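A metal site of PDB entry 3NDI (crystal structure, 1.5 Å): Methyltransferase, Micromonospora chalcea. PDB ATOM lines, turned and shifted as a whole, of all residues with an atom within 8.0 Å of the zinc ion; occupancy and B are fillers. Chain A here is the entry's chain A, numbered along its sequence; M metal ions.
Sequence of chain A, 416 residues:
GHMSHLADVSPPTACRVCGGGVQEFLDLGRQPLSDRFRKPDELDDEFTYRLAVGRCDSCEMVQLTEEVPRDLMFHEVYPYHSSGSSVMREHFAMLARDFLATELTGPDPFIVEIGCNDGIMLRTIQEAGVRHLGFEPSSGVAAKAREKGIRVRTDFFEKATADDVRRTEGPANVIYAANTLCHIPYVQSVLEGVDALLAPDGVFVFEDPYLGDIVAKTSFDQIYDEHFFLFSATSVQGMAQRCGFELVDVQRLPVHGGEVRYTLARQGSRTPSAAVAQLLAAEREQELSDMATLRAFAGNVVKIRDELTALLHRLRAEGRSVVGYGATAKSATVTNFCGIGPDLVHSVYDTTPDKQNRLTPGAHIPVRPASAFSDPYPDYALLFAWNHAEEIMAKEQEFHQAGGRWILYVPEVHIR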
ATOM      1  N   ALA A  14     -32.730   4.109  22.888  1.00  0.00           N
ATOM      2  CA  ALA A  14     -33.300   3.020  22.089  1.00  0.00           C
ATOM      3  C   ALA A  14     -32.271   2.407  21.118  1.00  0.00           C
ATOM      4  O   ALA A  14     -31.585   3.137  20.389  1.00  0.00           O
ATOM      5  CB  ALA A  14     -34.513   3.550  21.306  1.00  0.00           C
ATOM      6  N   CYS A  15     -32.138   1.083  21.103  1.00  0.00           N
ATOM      7  CA  CYS A  15     -31.246   0.451  20.111  1.00  0.00           C
ATOM      8  C   CYS A  15     -31.523   0.878  18.652  1.00  0.00           C
ATOM      9  O   CYS A  15     -32.666   0.922  18.197  1.00  0.00           O
ATOM     10  CB  CYS A  15     -31.364  -1.067  20.207  1.00  0.00           C
ATOM     11  SG  CYS A  15     -30.440  -2.102  19.008  1.00  0.00           S
ATOM     12  N   ARG A  16     -30.443   1.193  17.948  1.00  0.00           N
ATOM     13  CA  ARG A  16     -30.477   1.634  16.568  1.00  0.00           C
ATOM     14  C   ARG A  16     -30.815   0.500  15.622  1.00  0.00           C
ATOM     15  O   ARG A  16     -31.241   0.817  14.503  1.00  0.00           O
ATOM     16  CB  ARG A  16     -29.181   2.328  16.124  1.00  0.00           C
ATOM     17  CG  ARG A  16     -29.138   3.810  16.408  1.00  0.00           C
ATOM     18  CD  ARG A  16     -30.266   4.504  15.601  1.00  0.00           C
ATOM     19  NE  ARG A  16     -29.847   5.831  15.158  1.00  0.00           N
ATOM     20  CZ  ARG A  16     -30.232   6.409  14.025  1.00  0.00           C
ATOM     21  NH1 ARG A  16     -29.772   7.618  13.727  1.00  0.00           N
ATOM     22  NH2 ARG A  16     -31.075   5.805  13.185  1.00  0.00           N
ATOM     23  N   VAL A  17     -30.715  -0.740  16.084  1.00  0.00           N
ATOM     24  CA  VAL A  17     -31.029  -1.892  15.227  1.00  0.00           C
ATOM     25  C   VAL A  17     -32.494  -2.334  15.372  1.00  0.00           C
ATOM     26  O   VAL A  17     -33.187  -2.561  14.360  1.00  0.00           O
ATOM     27  CB  VAL A  17     -30.151  -3.164  15.462  1.00  0.00           C
ATOM     28  CG1 VAL A  17     -30.730  -4.424  14.763  1.00  0.00           C
ATOM     29  CG2 VAL A  17     -28.727  -2.877  15.017  1.00  0.00           C
ATOM     30  N   CYS A  18     -32.950  -2.495  16.610  1.00  0.00           N
ATOM     31  CA  CYS A  18     -34.212  -3.159  16.866  1.00  0.00           C
ATOM     32  C   CYS A  18     -35.164  -2.318  17.700  1.00  0.00           C
ATOM     33  O   CYS A  18     -36.291  -2.756  17.878  1.00  0.00           O
ATOM     34  CB  CYS A  18     -34.086  -4.558  17.474  1.00  0.00           C
ATOM     35  SG  CYS A  18     -33.581  -4.484  19.211  1.00  0.00           S
ATOM     36  N   GLY A  19     -34.731  -1.188  18.238  1.00  0.00           N
ATOM     37  CA  GLY A  19     -35.524  -0.398  19.170  1.00  0.00           C
ATOM     38  C   GLY A  19     -35.588  -0.860  20.621  1.00  0.00           C
ATOM     39  O   GLY A  19     -36.267  -0.202  21.414  1.00  0.00           O
ATOM     40  N   GLY A  20     -34.897  -1.936  20.966  1.00  0.00           N
ATOM     41  CA  GLY A  20     -34.839  -2.481  22.329  1.00  0.00           C
ATOM     42  C   GLY A  20     -34.144  -1.539  23.292  1.00  0.00           C
ATOM     43  O   GLY A  20     -33.598  -0.489  22.903  1.00  0.00           O
ATOM     44  N   GLY A  21     -34.150  -1.849  24.579  1.00  0.00           N
ATOM     45  CA  GLY A  21     -33.469  -0.935  25.486  1.00  0.00           C
ATOM     46  C   GLY A  21     -31.991  -1.235  25.609  1.00  0.00           C
ATOM     47  O   GLY A  21     -31.586  -2.402  25.672  1.00  0.00           O
ATOM     48  N   VAL A  22     -31.196  -0.178  25.652  1.00  0.00           N
ATOM     49  CA  VAL A  22     -29.735  -0.297  25.683  1.00  0.00           C
ATOM     50  C   VAL A  22     -29.240  -0.047  27.091  1.00  0.00           C
ATOM     51  O   VAL A  22     -29.469   1.023  27.656  1.00  0.00           O
ATOM     52  CB  VAL A  22     -29.104   0.754  24.726  1.00  0.00           C
ATOM     53  CG1 VAL A  22     -27.607   0.799  24.867  1.00  0.00           C
ATOM     54  CG2 VAL A  22     -29.421   0.360  23.263  1.00  0.00           C
ATOM     55  N   ARG A  55     -25.289  -2.038  25.709  1.00  0.00           N
ATOM     56  CA  ARG A  55     -25.592  -3.264  24.990  1.00  0.00           C
ATOM     57  C   ARG A  55     -27.116  -3.351  24.899  1.00  0.00           C
ATOM     58  O   ARG A  55     -27.788  -3.134  25.909  1.00  0.00           O
ATOM     59  CB  ARG A  55     -25.037  -4.491  25.739  1.00  0.00           C
ATOM     60  CG  ARG A  55     -25.300  -5.741  24.909  1.00  0.00           C
ATOM     61  CD  ARG A  55     -25.448  -7.007  25.709  1.00  0.00           C
ATOM     62  NE  ARG A  55     -26.741  -7.044  26.345  1.00  0.00           N
ATOM     63  CZ  ARG A  55     -27.086  -7.960  27.236  1.00  0.00           C
ATOM     64  NH1 ARG A  55     -28.301  -7.902  27.757  1.00  0.00           N
ATOM     65  NH2 ARG A  55     -26.204  -8.880  27.580  1.00  0.00           N
ATOM     66  N   CYS A  56     -27.679  -3.678  23.727  1.00  0.00           N
ATOM     67  CA  CYS A  56     -29.135  -3.718  23.636  1.00  0.00           C
ATOM     68  C   CYS A  56     -29.619  -4.990  24.340  1.00  0.00           C
ATOM     69  O   CYS A  56     -28.973  -6.018  24.207  1.00  0.00           O
ATOM     70  CB  CYS A  56     -29.557  -3.857  22.176  1.00  0.00           C
ATOM     71  SG  CYS A  56     -31.349  -4.150  21.907  1.00  0.00           S
ATOM     72  N   ASP A  57     -30.732  -4.924  25.056  1.00  0.00           N
ATOM     73  CA  ASP A  57     -31.263  -6.123  25.706  1.00  0.00           C
ATOM     74  C   ASP A  57     -31.920  -7.154  24.784  1.00  0.00           C
ATOM     75  O   ASP A  57     -32.028  -8.335  25.138  1.00  0.00           O
ATOM     76  CB  ASP A  57     -32.340  -5.743  26.727  1.00  0.00           C
ATOM     77  CG  ASP A  57     -31.774  -5.037  27.894  1.00  0.00           C
ATOM     78  OD1 ASP A  57     -30.581  -5.262  28.202  1.00  0.00           O
ATOM     79  OD2 ASP A  57     -32.576  -4.253  28.428  1.00  0.00           O
ATOM     80  N   SER A  58     -32.342  -6.753  23.599  1.00  0.00           N
ATOM     81  CA  SER A  58     -33.118  -7.679  22.774  1.00  0.00           C
ATOM     82  C   SER A  58     -32.249  -8.342  21.711  1.00  0.00           C
ATOM     83  O   SER A  58     -32.399  -9.502  21.396  1.00  0.00           O
ATOM     84  CB  SER A  58     -34.263  -6.920  22.114  1.00  0.00           C
ATOM     85  OG  SER A  58     -35.016  -6.285  23.121  1.00  0.00           O
ATOM     86  N   CYS A  59     -31.311  -7.595  21.130  1.00  0.00           N
ATOM     87  CA  CYS A  59     -30.489  -8.108  20.045  1.00  0.00           C
ATOM     88  C   CYS A  59     -28.984  -8.173  20.316  1.00  0.00           C
ATOM     89  O   CYS A  59     -28.224  -8.676  19.489  1.00  0.00           O
ATOM     90  CB  CYS A  59     -30.750  -7.305  18.774  1.00  0.00           C
ATOM     91  SG  CYS A  59     -29.792  -5.751  18.740  1.00  0.00           S
ATOM     92  N   GLU A  60     -28.615  -7.659  21.486  1.00  0.00           N
ATOM     93  CA  GLU A  60     -27.264  -7.790  21.999  1.00  0.00           C
ATOM     94  C   GLU A  60     -26.277  -6.905  21.241  1.00  0.00           C
ATOM     95  O   GLU A  60     -25.072  -7.074  21.446  1.00  0.00           O
ATOM     96  CB  GLU A  60     -26.806  -9.247  22.000  1.00  0.00           C
ATOM     97  CG  GLU A  60     -27.660 -10.110  22.953  1.00  0.00           C
ATOM     98  CD  GLU A  60     -27.170 -11.559  23.021  1.00  0.00           C
ATOM     99  OE1 GLU A  60     -26.137 -11.794  23.658  1.00  0.00           O
ATOM    100  OE2 GLU A  60     -27.815 -12.457  22.433  1.00  0.00           O
ATOM    101  N   MET A  61     -26.748  -5.970  20.431  1.00  0.00           N
ATOM    102  CA  MET A  61     -25.846  -5.045  19.729  1.00  0.00           C
ATOM    103  C   MET A  61     -25.215  -4.062  20.713  1.00  0.00           C
ATOM    104  O   MET A  61     -25.904  -3.357  21.473  1.00  0.00           O
ATOM    105  CB  MET A  61     -26.588  -4.312  18.618  1.00  0.00           C
ATOM    106  CG  MET A  61     -25.711  -3.323  17.862  1.00  0.00           C
ATOM    107  SD  MET A  61     -24.408  -4.189  16.960  1.00  0.00           S
ATOM    108  CE  MET A  61     -25.314  -4.839  15.575  1.00  0.00           C
ATOM    109  N   VAL A  62     -23.889  -4.047  20.732  1.00  0.00           N
ATOM    110  CA  VAL A  62     -23.144  -3.124  21.577  1.00  0.00           C
ATOM    111  C   VAL A  62     -22.935  -1.832  20.776  1.00  0.00           C
ATOM    112  O   VAL A  62     -22.563  -1.845  19.596  1.00  0.00           O
ATOM    113  CB  VAL A  62     -21.784  -3.755  21.846  1.00  0.00           C
ATOM    114  CG1 VAL A  62     -20.896  -2.747  22.529  1.00  0.00           C
ATOM    115  CG2 VAL A  62     -21.981  -4.950  22.778  1.00  0.00           C
ATOM    116  N   GLN A  63     -23.251  -0.688  21.380  1.00  0.00           N
ATOM    117  CA  GLN A  63     -23.345   0.566  20.666  1.00  0.00           C
ATOM    118  C   GLN A  63     -23.197   1.749  21.590  1.00  0.00           C
ATOM    119  O   GLN A  63     -23.464   1.644  22.778  1.00  0.00           O
ATOM    120  CB  GLN A  63     -24.696   0.684  19.913  1.00  0.00           C
ATOM    121  CG  GLN A  63     -25.944   0.763  20.823  1.00  0.00           C
ATOM    122  CD  GLN A  63     -27.176   0.299  20.083  1.00  0.00           C
ATOM    123  OE1 GLN A  63     -27.867   1.143  19.469  1.00  0.00           O
ATOM    124  NE2 GLN A  63     -27.507  -0.988  20.184  1.00  0.00           N
ATOM    125  N   PHE A 229     -20.852   1.269  16.556  1.00  0.00           N
ATOM    126  CA  PHE A 229     -21.167  -0.130  16.825  1.00  0.00           C
ATOM    127  C   PHE A 229     -19.916  -0.925  17.107  1.00  0.00           C
ATOM    128  O   PHE A 229     -18.915  -0.734  16.412  1.00  0.00           O
ATOM    129  CB  PHE A 229     -21.903  -0.799  15.658  1.00  0.00           C
ATOM    130  CG  PHE A 229     -23.298  -0.302  15.439  1.00  0.00           C
ATOM    131  CD1 PHE A 229     -24.270  -0.544  16.396  1.00  0.00           C
ATOM    132  CD2 PHE A 229     -23.594   0.405  14.290  1.00  0.00           C
ATOM    133  CE1 PHE A 229     -25.559  -0.052  16.180  1.00  0.00           C
ATOM    134  CE2 PHE A 229     -24.877   0.877  14.080  1.00  0.00           C
ATOM    135  CZ  PHE A 229     -25.865   0.640  15.018  1.00  0.00           C
ATOM    136  N   SER A 235     -24.580 -10.353  17.400  1.00  0.00           N
ATOM    137  CA  SER A 235     -25.372  -9.171  17.018  1.00  0.00           C
ATOM    138  C   SER A 235     -25.568  -8.978  15.501  1.00  0.00           C
ATOM    139  O   SER A 235     -26.649  -8.586  15.048  1.00  0.00           O
ATOM    140  CB  SER A 235     -24.858  -7.884  17.685  1.00  0.00           C
ATOM    141  OG  SER A 235     -23.581  -7.536  17.169  1.00  0.00           O
ATOM    142  N   MET A 239     -29.015  -8.739  13.473  1.00  0.00           N
ATOM    143  CA  MET A 239     -29.243  -7.568  12.639  1.00  0.00           C
ATOM    144  C   MET A 239     -29.615  -7.960  11.218  1.00  0.00           C
ATOM    145  O   MET A 239     -30.542  -7.426  10.610  1.00  0.00           O
ATOM    146  CB  MET A 239     -27.968  -6.734  12.570  1.00  0.00           C
ATOM    147  CG  MET A 239     -28.168  -5.473  11.722  1.00  0.00           C
ATOM    148  SD  MET A 239     -26.698  -4.404  11.763  1.00  0.00           S
ATOM    149  CE  MET A 239     -25.467  -5.266  10.775  1.00  0.00           C
ATOM    150  N   ARG A 242     -33.157  -9.557  11.235  1.00  0.00           N
ATOM    151  CA  ARG A 242     -34.270  -8.651  11.519  1.00  0.00           C
ATOM    152  C   ARG A 242     -34.503  -7.681  10.376  1.00  0.00           C
ATOM    153  O   ARG A 242     -35.475  -6.914  10.381  1.00  0.00           O
ATOM    154  CB  ARG A 242     -33.994  -7.846  12.789  1.00  0.00           C
ATOM    155  CG  ARG A 242     -34.074  -8.599  14.106  1.00  0.00           C
ATOM    156  CD  ARG A 242     -33.520  -7.662  15.186  1.00  0.00           C
ATOM    157  NE  ARG A 242     -33.576  -8.233  16.527  1.00  0.00           N
ATOM    158  CZ  ARG A 242     -34.655  -8.216  17.310  1.00  0.00           C
ATOM    159  NH1 ARG A 242     -35.796  -7.689  16.886  1.00  0.00           N
ATOM    160  NH2 ARG A 242     -34.563  -8.742  18.519  1.00  0.00           N
HETATM  161 ZN    ZN M   1     -31.311  -4.164  19.566  1.00  0.00          ZN
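Within 4 Å of the zinc ion: Cys 15, Cys 18, Cys 56 and Cys 59.
Along chain A the residues within 4 Å of the zinc ion span positions 15 to 59.
The zinc ion is bound by the side-chain sulfur of Cys 15 (2.3 Å), the side-chain sulfur of Cys 18 (2.3 Å), the side-chain sulfur of Cys 56 (2.3 Å) and the side-chain sulfur of Cys 59 (2.3 Å).
The zinc ion has four donor atoms within binding distance.
The side-chain sulfur (SG) of Cys 59 sits close to the backbone NH (N) of Met 61.
The backbone NH (N) of Val 17 lies close to the side-chain sulfur (SG) of Cys 15 (3.2 Å).
The backbone NH (N) of Gly 20 lies close to the side-chain sulfur (SG) of Cys 18 (3.4 Å).
O of Met 61 lies within hydrogen-bond range of N of Cys 56 (2.9 Å).
SG of Cys 15 sits close to NE2 of Gln 63 (3.4 Å).
The backbone NH of Ser 58 lies close to the side-chain sulfur of Cys 56, at 3.3 Å.
The backbone carbonyl oxygen (O) of Gly 20 lies within hydrogen-bond range of the backbone NH (N) of Cys 15, at 2.8 Å.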
